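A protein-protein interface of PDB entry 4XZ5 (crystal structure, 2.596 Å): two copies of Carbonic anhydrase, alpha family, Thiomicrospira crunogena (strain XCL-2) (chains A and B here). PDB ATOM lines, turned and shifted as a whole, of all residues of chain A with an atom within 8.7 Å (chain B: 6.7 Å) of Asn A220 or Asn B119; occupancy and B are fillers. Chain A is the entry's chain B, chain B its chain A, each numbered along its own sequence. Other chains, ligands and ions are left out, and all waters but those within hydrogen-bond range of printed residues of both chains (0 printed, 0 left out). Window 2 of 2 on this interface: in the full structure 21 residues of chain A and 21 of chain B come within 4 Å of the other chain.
OG of Ser B174 sits at hydrogen-bond distance from OD1 of Asn A30 (3.2 Å).
The backbone carbonyl oxygen (O) of Ala A221 lies within hydrogen-bond range of the side-chain amino group (NZ) of Lys B172 (2.5 Å).
The side-chain hydroxyl (OG1) of Thr A223 sits close to the side-chain amino group (NZ) of Lys B172, at 3.2 Å.
The backbone carbonyl oxygen (O) of Leu B120 lies within hydrogen-bond range of the backbone NH (N) of Tyr B187, 2.9 Å away.
O of Arg A218 lies within hydrogen-bond range of ND2 of Asn A220.
O of Arg A218 is in hydrogen-bond range of NH2 of Arg A222.
O of Gln A31 lies within hydrogen-bond range of NH1 of Arg A222 (2.8 Å).
The backbone NH of Asn A30 sits at hydrogen-bond distance from the side-chain carboxylate of Glu A184 (3.3 Å).
ND2 of Asn A220 lies within hydrogen-bond range of O of Lys A29, at 2.9 Å.
Among the printed residues, pairs that only touch across the chains: Lys A29 with Gly B185 (3.7 Å), Asn A220 with Asn B119 (3.9 Å), Ala A221 with Ser B174 (3.7 Å), Ala A221 with Gly B185 (3.2 Å), Ala A221 with Val B186 (3.4 Å), Ala A221 with Tyr B187 (3.5 Å) and Arg A222 with Ser B174 (3.95 Å).
Of chain A, only Asn A220 comes within 4 Å of Asn B119.
Gly B118 touches none of the printed residues of chain A.
Printed residues of chain B within 4 Å of Thr A223: Lys B172.
Printed residues of chain A within 4 Å of Val B186: Ala A221.
Of the printed residues of chain B, Lys A29 touches Gly B185 (3.7 Å).
Of the printed residues of chain B, Asn A30 touches Ser B174 (3.2 Å).
Of the printed residues of chain B, Arg A222 touches Ser B174.
Thr A27 touches none of the printed residues of chain B.
The nearest residue of chain B that does not touch Asn A220 is Gly B185 (4.7 Å).
The nearest residue of chain A that does not touch Asn B119 is Ala A221 (5.4 Å).
The nearest printed residue of chain B that does not touch Lys A29 is Ser B174 (5.9 Å).
Of the 15 printed residues of chain A, 6 touch a printed residue of chain B.
Printed residues of chain A that touch a printed residue of chain B: Lys A29, Asn A30, Asn A220, Ala A221, Arg A222 and Thr A223.
No position is printed for both chains.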
ATOM      1  N   THR A  27     -14.841  15.371 -28.365  1.00  0.00           N
ATOM      2  CA  THR A  27     -14.445  15.476 -26.961  1.00  0.00           C
ATOM      3  C   THR A  27     -13.690  14.238 -26.467  1.00  0.00           C
ATOM      4  O   THR A  27     -13.156  14.221 -25.355  1.00  0.00           O
ATOM      5  CB  THR A  27     -15.670  15.706 -26.026  1.00  0.00           C
ATOM      6  OG1 THR A  27     -16.574  14.607 -26.130  1.00  0.00           O
ATOM      7  CG2 THR A  27     -16.414  16.974 -26.389  1.00  0.00           C
ATOM      8  N   GLY A  28     -13.636  13.206 -27.302  1.00  0.00           N
ATOM      9  CA  GLY A  28     -13.057  11.938 -26.906  1.00  0.00           C
ATOM     10  C   GLY A  28     -11.550  11.962 -26.750  1.00  0.00           C
ATOM     11  O   GLY A  28     -10.838  12.664 -27.464  1.00  0.00           O
ATOM     12  N   LYS A  29     -11.066  11.180 -25.795  1.00  0.00           N
ATOM     13  CA  LYS A  29      -9.643  11.095 -25.553  1.00  0.00           C
ATOM     14  C   LYS A  29      -9.076   9.735 -25.920  1.00  0.00           C
ATOM     15  O   LYS A  29      -7.869   9.518 -25.879  1.00  0.00           O
ATOM     16  CB  LYS A  29      -9.388  11.405 -24.096  1.00  0.00           C
ATOM     17  CG  LYS A  29      -9.868  12.790 -23.727  1.00  0.00           C
ATOM     18  CD  LYS A  29      -8.947  13.848 -24.307  1.00  0.00           C
ATOM     19  CE  LYS A  29      -9.573  15.222 -24.263  1.00  0.00           C
ATOM     20  NZ  LYS A  29      -8.657  16.184 -24.904  1.00  0.00           N
ATOM     21  N   ASN A  30      -9.957   8.841 -26.346  1.00  0.00           N
ATOM     22  CA  ASN A  30      -9.567   7.500 -26.737  1.00  0.00           C
ATOM     23  C   ASN A  30     -10.172   7.154 -28.101  1.00  0.00           C
ATOM     24  O   ASN A  30     -10.904   6.169 -28.249  1.00  0.00           O
ATOM     25  CB  ASN A  30     -10.011   6.490 -25.678  1.00  0.00           C
ATOM     26  CG  ASN A  30      -9.448   6.789 -24.306  1.00  0.00           C
ATOM     27  OD1 ASN A  30      -8.407   6.261 -23.928  1.00  0.00           O
ATOM     28  ND2 ASN A  30     -10.144   7.630 -23.545  1.00  0.00           N
ATOM     29  N   GLN A  31      -9.846   7.975 -29.096  1.00  0.00           N
ATOM     30  CA  GLN A  31     -10.463   7.888 -30.410  1.00  0.00           C
ATOM     31  C   GLN A  31      -9.617   7.065 -31.361  1.00  0.00           C
ATOM     32  O   GLN A  31      -8.414   6.901 -31.162  1.00  0.00           O
ATOM     33  CB  GLN A  31     -10.691   9.287 -31.000  1.00  0.00           C
ATOM     34  CG  GLN A  31     -11.748  10.103 -30.275  1.00  0.00           C
ATOM     35  CD  GLN A  31     -13.158   9.634 -30.606  1.00  0.00           C
ATOM     36  OE1 GLN A  31     -13.654   9.845 -31.717  1.00  0.00           O
ATOM     37  NE2 GLN A  31     -13.809   8.987 -29.642  1.00  0.00           N
ATOM     38  N   ILE A  34      -5.370   5.511 -34.965  1.00  0.00           N
ATOM     39  CA  ILE A  34      -4.133   6.116 -34.515  1.00  0.00           C
ATOM     40  C   ILE A  34      -2.990   5.799 -35.447  1.00  0.00           C
ATOM     41  O   ILE A  34      -3.048   4.833 -36.212  1.00  0.00           O
ATOM     42  CB  ILE A  34      -3.767   5.641 -33.123  1.00  0.00           C
ATOM     43  CG1 ILE A  34      -3.748   4.111 -33.116  1.00  0.00           C
ATOM     44  CG2 ILE A  34      -4.767   6.169 -32.107  1.00  0.00           C
ATOM     45  CD1 ILE A  34      -3.046   3.528 -31.963  1.00  0.00           C
ATOM     46  N   GLU A 184     -16.890   5.258 -28.002  1.00  0.00           N
ATOM     47  CA  GLU A 184     -15.664   4.746 -27.435  1.00  0.00           C
ATOM     48  C   GLU A 184     -15.915   3.409 -26.748  1.00  0.00           C
ATOM     49  O   GLU A 184     -17.052   2.948 -26.690  1.00  0.00           O
ATOM     50  CB  GLU A 184     -15.069   5.774 -26.474  1.00  0.00           C
ATOM     51  CG  GLU A 184     -13.941   6.559 -27.098  1.00  0.00           C
ATOM     52  CD  GLU A 184     -13.582   7.820 -26.350  1.00  0.00           C
ATOM     53  OE1 GLU A 184     -13.599   7.807 -25.096  1.00  0.00           O
ATOM     54  OE2 GLU A 184     -13.233   8.810 -27.029  1.00  0.00           O
ATOM     55  N   GLN A 217      -5.925   9.957 -34.909  1.00  0.00           N
ATOM     56  CA  GLN A 217      -6.259  10.644 -33.660  1.00  0.00           C
ATOM     57  C   GLN A 217      -5.115  10.521 -32.668  1.00  0.00           C
ATOM     58  O   GLN A 217      -4.254   9.648 -32.817  1.00  0.00           O
ATOM     59  CB  GLN A 217      -7.550  10.080 -33.052  1.00  0.00           C
ATOM     60  CG  GLN A 217      -8.726  10.067 -34.011  1.00  0.00           C
ATOM     61  CD  GLN A 217      -9.233  11.454 -34.317  1.00  0.00           C
ATOM     62  OE1 GLN A 217      -9.606  12.196 -33.416  1.00  0.00           O
ATOM     63  NE2 GLN A 217      -9.214  11.824 -35.584  1.00  0.00           N
ATOM     64  N   ARG A 218      -5.109  11.406 -31.668  1.00  0.00           N
ATOM     65  CA  ARG A 218      -4.060  11.419 -30.646  1.00  0.00           C
ATOM     66  C   ARG A 218      -4.102  10.155 -29.781  1.00  0.00           C
ATOM     67  O   ARG A 218      -5.173   9.740 -29.307  1.00  0.00           O
ATOM     68  CB  ARG A 218      -4.199  12.632 -29.722  1.00  0.00           C
ATOM     69  CG  ARG A 218      -3.910  13.967 -30.365  1.00  0.00           C
ATOM     70  CD  ARG A 218      -3.830  15.090 -29.331  1.00  0.00           C
ATOM     71  NE  ARG A 218      -3.998  16.393 -29.972  1.00  0.00           N
ATOM     72  CZ  ARG A 218      -3.005  17.135 -30.465  1.00  0.00           C
ATOM     73  NH1 ARG A 218      -1.747  16.703 -30.425  1.00  0.00           N
ATOM     74  NH2 ARG A 218      -3.276  18.307 -31.026  1.00  0.00           N
ATOM     75  N   GLN A 219      -2.936   9.561 -29.554  1.00  0.00           N
ATOM     76  CA  GLN A 219      -2.852   8.390 -28.702  1.00  0.00           C
ATOM     77  C   GLN A 219      -3.177   8.755 -27.240  1.00  0.00           C
ATOM     78  O   GLN A 219      -3.767   7.955 -26.504  1.00  0.00           O
ATOM     79  CB  GLN A 219      -1.478   7.750 -28.820  1.00  0.00           C
ATOM     80  CG  GLN A 219      -1.354   6.434 -28.089  1.00  0.00           C
ATOM     81  CD  GLN A 219      -0.260   5.553 -28.653  1.00  0.00           C
ATOM     82  OE1 GLN A 219      -0.021   5.528 -29.865  1.00  0.00           O
ATOM     83  NE2 GLN A 219       0.420   4.832 -27.775  1.00  0.00           N
ATOM     84  N   ASN A 220      -2.805   9.971 -26.843  1.00  0.00           N
ATOM     85  CA  ASN A 220      -3.042  10.486 -25.488  1.00  0.00           C
ATOM     86  C   ASN A 220      -2.478   9.566 -24.409  1.00  0.00           C
ATOM     87  O   ASN A 220      -1.279   9.264 -24.403  1.00  0.00           O
ATOM     88  CB  ASN A 220      -4.531  10.737 -25.277  1.00  0.00           C
ATOM     89  CG  ASN A 220      -5.034  11.907 -26.080  1.00  0.00           C
ATOM     90  OD1 ASN A 220      -4.361  12.928 -26.193  1.00  0.00           O
ATOM     91  ND2 ASN A 220      -6.201  11.753 -26.681  1.00  0.00           N
ATOM     92  N   ALA A 221      -3.329   9.132 -23.490  1.00  0.00           N
ATOM     93  CA  ALA A 221      -2.863   8.344 -22.360  1.00  0.00           C
ATOM     94  C   ALA A 221      -2.739   6.841 -22.652  1.00  0.00           C
ATOM     95  O   ALA A 221      -2.436   6.051 -21.751  1.00  0.00           O
ATOM     96  CB  ALA A 221      -3.791   8.574 -21.169  1.00  0.00           C
ATOM     97  N   ARG A 222      -2.983   6.445 -23.896  1.00  0.00           N
ATOM     98  CA  ARG A 222      -3.025   5.018 -24.242  1.00  0.00           C
ATOM     99  C   ARG A 222      -1.650   4.431 -24.525  1.00  0.00           C
ATOM    100  O   ARG A 222      -0.750   5.106 -25.039  1.00  0.00           O
ATOM    101  CB  ARG A 222      -3.952   4.784 -25.446  1.00  0.00           C
ATOM    102  CG  ARG A 222      -5.431   5.042 -25.160  1.00  0.00           C
ATOM    103  CD  ARG A 222      -6.300   4.969 -26.407  1.00  0.00           C
ATOM    104  NE  ARG A 222      -6.016   6.074 -27.320  1.00  0.00           N
ATOM    105  CZ  ARG A 222      -6.664   6.294 -28.457  1.00  0.00           C
ATOM    106  NH1 ARG A 222      -7.664   5.515 -28.807  1.00  0.00           N
ATOM    107  NH2 ARG A 222      -6.333   7.318 -29.228  1.00  0.00           N
ATOM    108  N   THR A 223      -1.494   3.168 -24.153  1.00  0.00           N
ATOM    109  CA  THR A 223      -0.325   2.377 -24.518  1.00  0.00           C
ATOM    110  C   THR A 223      -0.688   1.445 -25.684  1.00  0.00           C
ATOM    111  O   THR A 223      -1.721   0.788 -25.661  1.00  0.00           O
ATOM    112  CB  THR A 223       0.178   1.558 -23.324  1.00  0.00           C
ATOM    113  OG1 THR A 223       0.644   2.452 -22.303  1.00  0.00           O
ATOM    114  CG2 THR A 223       1.295   0.627 -23.752  1.00  0.00           C
ATOM    115  N   LEU A 224       0.130   1.409 -26.722  1.00  0.00           N
ATOM    116  CA  LEU A 224      -0.110   0.481 -27.820  1.00  0.00           C
ATOM    117  C   LEU A 224       0.535  -0.884 -27.489  1.00  0.00           C
ATOM    118  O   LEU A 224       1.737  -0.953 -27.248  1.00  0.00           O
ATOM    119  CB  LEU A 224       0.431   1.061 -29.149  1.00  0.00           C
ATOM    120  CG  LEU A 224       0.222   0.200 -30.421  1.00  0.00           C
ATOM    121  CD1 LEU A 224      -1.259   0.023 -30.751  1.00  0.00           C
ATOM    122  CD2 LEU A 224       0.978   0.740 -31.646  1.00  0.00           C
ATOM    123  N   HIS B  83       9.731  11.574 -21.514  1.00  0.00           N
ATOM    124  CA  HIS B  83       8.637  12.536 -21.584  1.00  0.00           C
ATOM    125  C   HIS B  83       8.366  13.104 -20.178  1.00  0.00           C
ATOM    126  O   HIS B  83       8.162  12.351 -19.208  1.00  0.00           O
ATOM    127  CB  HIS B  83       7.392  11.864 -22.155  1.00  0.00           C
ATOM    128  CG  HIS B  83       6.227  12.786 -22.342  1.00  0.00           C
ATOM    129  ND1 HIS B  83       4.928  12.330 -22.417  1.00  0.00           N
ATOM    130  CD2 HIS B  83       6.162  14.130 -22.487  1.00  0.00           C
ATOM    131  CE1 HIS B  83       4.111  13.355 -22.584  1.00  0.00           C
ATOM    132  NE2 HIS B  83       4.836  14.459 -22.631  1.00  0.00           N
ATOM    133  N   TYR B  85       6.616  15.281 -17.090  1.00  0.00           N
ATOM    134  CA  TYR B  85       5.374  15.803 -16.489  1.00  0.00           C
ATOM    135  C   TYR B  85       5.686  16.514 -15.155  1.00  0.00           C
ATOM    136  O   TYR B  85       6.444  15.992 -14.346  1.00  0.00           O
ATOM    137  CB  TYR B  85       4.378  14.682 -16.226  1.00  0.00           C
ATOM    138  CG  TYR B  85       3.907  13.839 -17.415  1.00  0.00           C
ATOM    139  CD1 TYR B  85       2.592  13.934 -17.895  1.00  0.00           C
ATOM    140  CD2 TYR B  85       4.738  12.887 -17.984  1.00  0.00           C
ATOM    141  CE1 TYR B  85       2.155  13.140 -18.932  1.00  0.00           C
ATOM    142  CE2 TYR B  85       4.309  12.089 -19.029  1.00  0.00           C
ATOM    143  CZ  TYR B  85       3.022  12.216 -19.501  1.00  0.00           C
ATOM    144  OH  TYR B  85       2.615  11.408 -20.542  1.00  0.00           O
ATOM    145  N   HIS B 113       0.291  14.811 -11.971  1.00  0.00           N
ATOM    146  CA  HIS B 113       1.257  15.433 -12.887  1.00  0.00           C
ATOM    147  C   HIS B 113       0.636  15.909 -14.216  1.00  0.00           C
ATOM    148  O   HIS B 113      -0.318  15.307 -14.725  1.00  0.00           O
ATOM    149  CB  HIS B 113       2.406  14.476 -13.226  1.00  0.00           C
ATOM    150  CG  HIS B 113       3.050  13.830 -12.046  1.00  0.00           C
ATOM    151  ND1 HIS B 113       2.433  12.844 -11.307  1.00  0.00           N
ATOM    152  CD2 HIS B 113       4.281  13.988 -11.505  1.00  0.00           C
ATOM    153  CE1 HIS B 113       3.248  12.435 -10.352  1.00  0.00           C
ATOM    154  NE2 HIS B 113       4.374  13.117 -10.449  1.00  0.00           N
ATOM    155  N   LYS B 114       1.202  16.978 -14.776  1.00  0.00           N
ATOM    156  CA  LYS B 114       0.761  17.506 -16.064  1.00  0.00           C
ATOM    157  C   LYS B 114       1.961  17.911 -16.949  1.00  0.00           C
ATOM    158  O   LYS B 114       2.951  18.458 -16.449  1.00  0.00           O
ATOM    159  CB  LYS B 114      -0.194  18.686 -15.857  1.00  0.00           C
ATOM    160  CG  LYS B 114      -0.680  19.316 -17.156  1.00  0.00           C
ATOM    161  CD  LYS B 114      -2.027  20.001 -17.011  1.00  0.00           C
ATOM    162  CE  LYS B 114      -1.937  21.232 -16.162  1.00  0.00           C
ATOM    163  NZ  LYS B 114      -2.988  22.185 -16.571  1.00  0.00           N
ATOM    164  N   ASP B 115       1.877  17.633 -18.256  1.00  0.00           N
ATOM    165  CA  ASP B 115       2.940  18.044 -19.178  1.00  0.00           C
ATOM    166  C   ASP B 115       2.580  19.355 -19.843  1.00  0.00           C
ATOM    167  O   ASP B 115       1.576  19.974 -19.477  1.00  0.00           O
ATOM    168  CB  ASP B 115       3.246  16.958 -20.231  1.00  0.00           C
ATOM    169  CG  ASP B 115       2.143  16.773 -21.288  1.00  0.00           C
ATOM    170  OD1 ASP B 115       1.145  17.534 -21.354  1.00  0.00           O
ATOM    171  OD2 ASP B 115       2.288  15.811 -22.075  1.00  0.00           O
ATOM    172  N   GLY B 116       3.411  19.776 -20.799  1.00  0.00           N
ATOM    173  CA  GLY B 116       3.201  21.007 -21.551  1.00  0.00           C
ATOM    174  C   GLY B 116       1.906  21.118 -22.354  1.00  0.00           C
ATOM    175  O   GLY B 116       1.382  22.218 -22.513  1.00  0.00           O
ATOM    176  N   ASP B 117       1.396  19.996 -22.864  1.00  0.00           N
ATOM    177  CA  ASP B 117       0.168  19.974 -23.682  1.00  0.00           C
ATOM    178  C   ASP B 117      -1.137  19.731 -22.915  1.00  0.00           C
ATOM    179  O   ASP B 117      -2.198  19.564 -23.521  1.00  0.00           O
ATOM    180  CB  ASP B 117       0.272  18.931 -24.792  1.00  0.00           C
ATOM    181  CG  ASP B 117       1.201  19.362 -25.895  1.00  0.00           C
ATOM    182  OD1 ASP B 117       1.137  20.548 -26.286  1.00  0.00           O
ATOM    183  OD2 ASP B 117       1.971  18.517 -26.393  1.00  0.00           O
ATOM    184  N   GLY B 118      -1.053  19.622 -21.598  1.00  0.00           N
ATOM    185  CA  GLY B 118      -2.246  19.434 -20.801  1.00  0.00           C
ATOM    186  C   GLY B 118      -2.514  17.997 -20.398  1.00  0.00           C
ATOM    187  O   GLY B 118      -3.452  17.742 -19.651  1.00  0.00           O
ATOM    188  N   ASN B 119      -1.684  17.076 -20.881  1.00  0.00           N
ATOM    189  CA  ASN B 119      -1.771  15.663 -20.532  1.00  0.00           C
ATOM    190  C   ASN B 119      -1.509  15.407 -19.069  1.00  0.00           C
ATOM    191  O   ASN B 119      -0.596  15.993 -18.480  1.00  0.00           O
ATOM    192  CB  ASN B 119      -0.781  14.853 -21.349  1.00  0.00           C
ATOM    193  CG  ASN B 119      -1.047  14.940 -22.816  1.00  0.00           C
ATOM    194  OD1 ASN B 119      -0.260  15.514 -23.563  1.00  0.00           O
ATOM    195  ND2 ASN B 119      -2.164  14.362 -23.248  1.00  0.00           N
ATOM    196  N   LEU B 120      -2.291  14.502 -18.495  1.00  0.00           N
ATOM    197  CA  LEU B 120      -2.220  14.227 -17.067  1.00  0.00           C
ATOM    198  C   LEU B 120      -1.619  12.841 -16.836  1.00  0.00           C
ATOM    199  O   LEU B 120      -1.921  11.893 -17.558  1.00  0.00           O
ATOM    200  CB  LEU B 120      -3.605  14.297 -16.442  1.00  0.00           C
ATOM    201  CG  LEU B 120      -4.158  15.691 -16.142  1.00  0.00           C
ATOM    202  CD1 LEU B 120      -5.613  15.541 -15.683  1.00  0.00           C
ATOM    203  CD2 LEU B 120      -3.318  16.550 -15.181  1.00  0.00           C
ATOM    204  N   ALA B 121      -0.747  12.730 -15.849  1.00  0.00           N
ATOM    205  CA  ALA B 121      -0.237  11.438 -15.437  1.00  0.00           C
ATOM    206  C   ALA B 121      -0.389  11.355 -13.936  1.00  0.00           C
ATOM    207  O   ALA B 121       0.006  12.277 -13.231  1.00  0.00           O
ATOM    208  CB  ALA B 121       1.219  11.270 -15.850  1.00  0.00           C
ATOM    209  N   LYS B 172      -0.507  -0.137 -14.935  1.00  0.00           N
ATOM    210  CA  LYS B 172      -0.793   1.079 -15.695  1.00  0.00           C
ATOM    211  C   LYS B 172      -2.022   0.878 -16.584  1.00  0.00           C
ATOM    212  O   LYS B 172      -2.244  -0.206 -17.116  1.00  0.00           O
ATOM    213  CB  LYS B 172       0.457   1.530 -16.494  1.00  0.00           C
ATOM    214  CG  LYS B 172       0.262   1.810 -17.993  1.00  0.00           C
ATOM    215  CD  LYS B 172      -0.369   3.140 -18.344  1.00  0.00           C
ATOM    216  CE  LYS B 172      -1.033   3.016 -19.704  1.00  0.00           C
ATOM    217  NZ  LYS B 172      -1.165   4.287 -20.442  1.00  0.00           N
ATOM    218  N   SER B 174      -5.183   3.464 -19.022  1.00  0.00           N
ATOM    219  CA  SER B 174      -5.648   4.751 -19.474  1.00  0.00           C
ATOM    220  C   SER B 174      -6.970   5.061 -18.798  1.00  0.00           C
ATOM    221  O   SER B 174      -7.927   4.314 -18.941  1.00  0.00           O
ATOM    222  CB  SER B 174      -5.785   4.766 -21.003  1.00  0.00           C
ATOM    223  OG  SER B 174      -6.435   5.943 -21.445  1.00  0.00           O
ATOM    224  N   GLY B 185      -8.192  10.700 -20.622  1.00  0.00           N
ATOM    225  CA  GLY B 185      -6.881  10.923 -21.201  1.00  0.00           C
ATOM    226  C   GLY B 185      -5.833  10.969 -20.110  1.00  0.00           C
ATOM    227  O   GLY B 185      -4.758  11.538 -20.290  1.00  0.00           O
ATOM    228  N   VAL B 186      -6.155  10.368 -18.965  1.00  0.00           N
ATOM    229  CA  VAL B 186      -5.236  10.358 -17.830  1.00  0.00           C
ATOM    230  C   VAL B 186      -4.415   9.073 -17.818  1.00  0.00           C
ATOM    231  O   VAL B 186      -4.957   7.964 -17.880  1.00  0.00           O
ATOM    232  CB  VAL B 186      -5.980  10.501 -16.468  1.00  0.00           C
ATOM    233  CG1 VAL B 186      -4.980  10.531 -15.312  1.00  0.00           C
ATOM    234  CG2 VAL B 186      -6.843  11.757 -16.442  1.00  0.00           C
ATOM    235  N   TYR B 187      -3.101   9.244 -17.752  1.00  0.00           N
ATOM    236  CA  TYR B 187      -2.154   8.148 -17.644  1.00  0.00           C
ATOM    237  C   TYR B 187      -2.032   7.678 -16.168  1.00  0.00           C
ATOM    238  O   TYR B 187      -1.440   8.371 -15.345  1.00  0.00           O
ATOM    239  CB  TYR B 187      -0.807   8.626 -18.171  1.00  0.00           C
ATOM    240  CG  TYR B 187       0.214   7.571 -18.517  1.00  0.00           C
ATOM    241  CD1 TYR B 187       0.987   6.960 -17.527  1.00  0.00           C
ATOM    242  CD2 TYR B 187       0.459   7.225 -19.856  1.00  0.00           C
ATOM    243  CE1 TYR B 187       1.955   6.002 -17.859  1.00  0.00           C
ATOM    244  CE2 TYR B 187       1.424   6.282 -20.195  1.00  0.00           C
ATOM    245  CZ  TYR B 187       2.171   5.680 -19.196  1.00  0.00           C
ATOM    246  OH  TYR B 187       3.130   4.750 -19.533  1.00  0.00           O
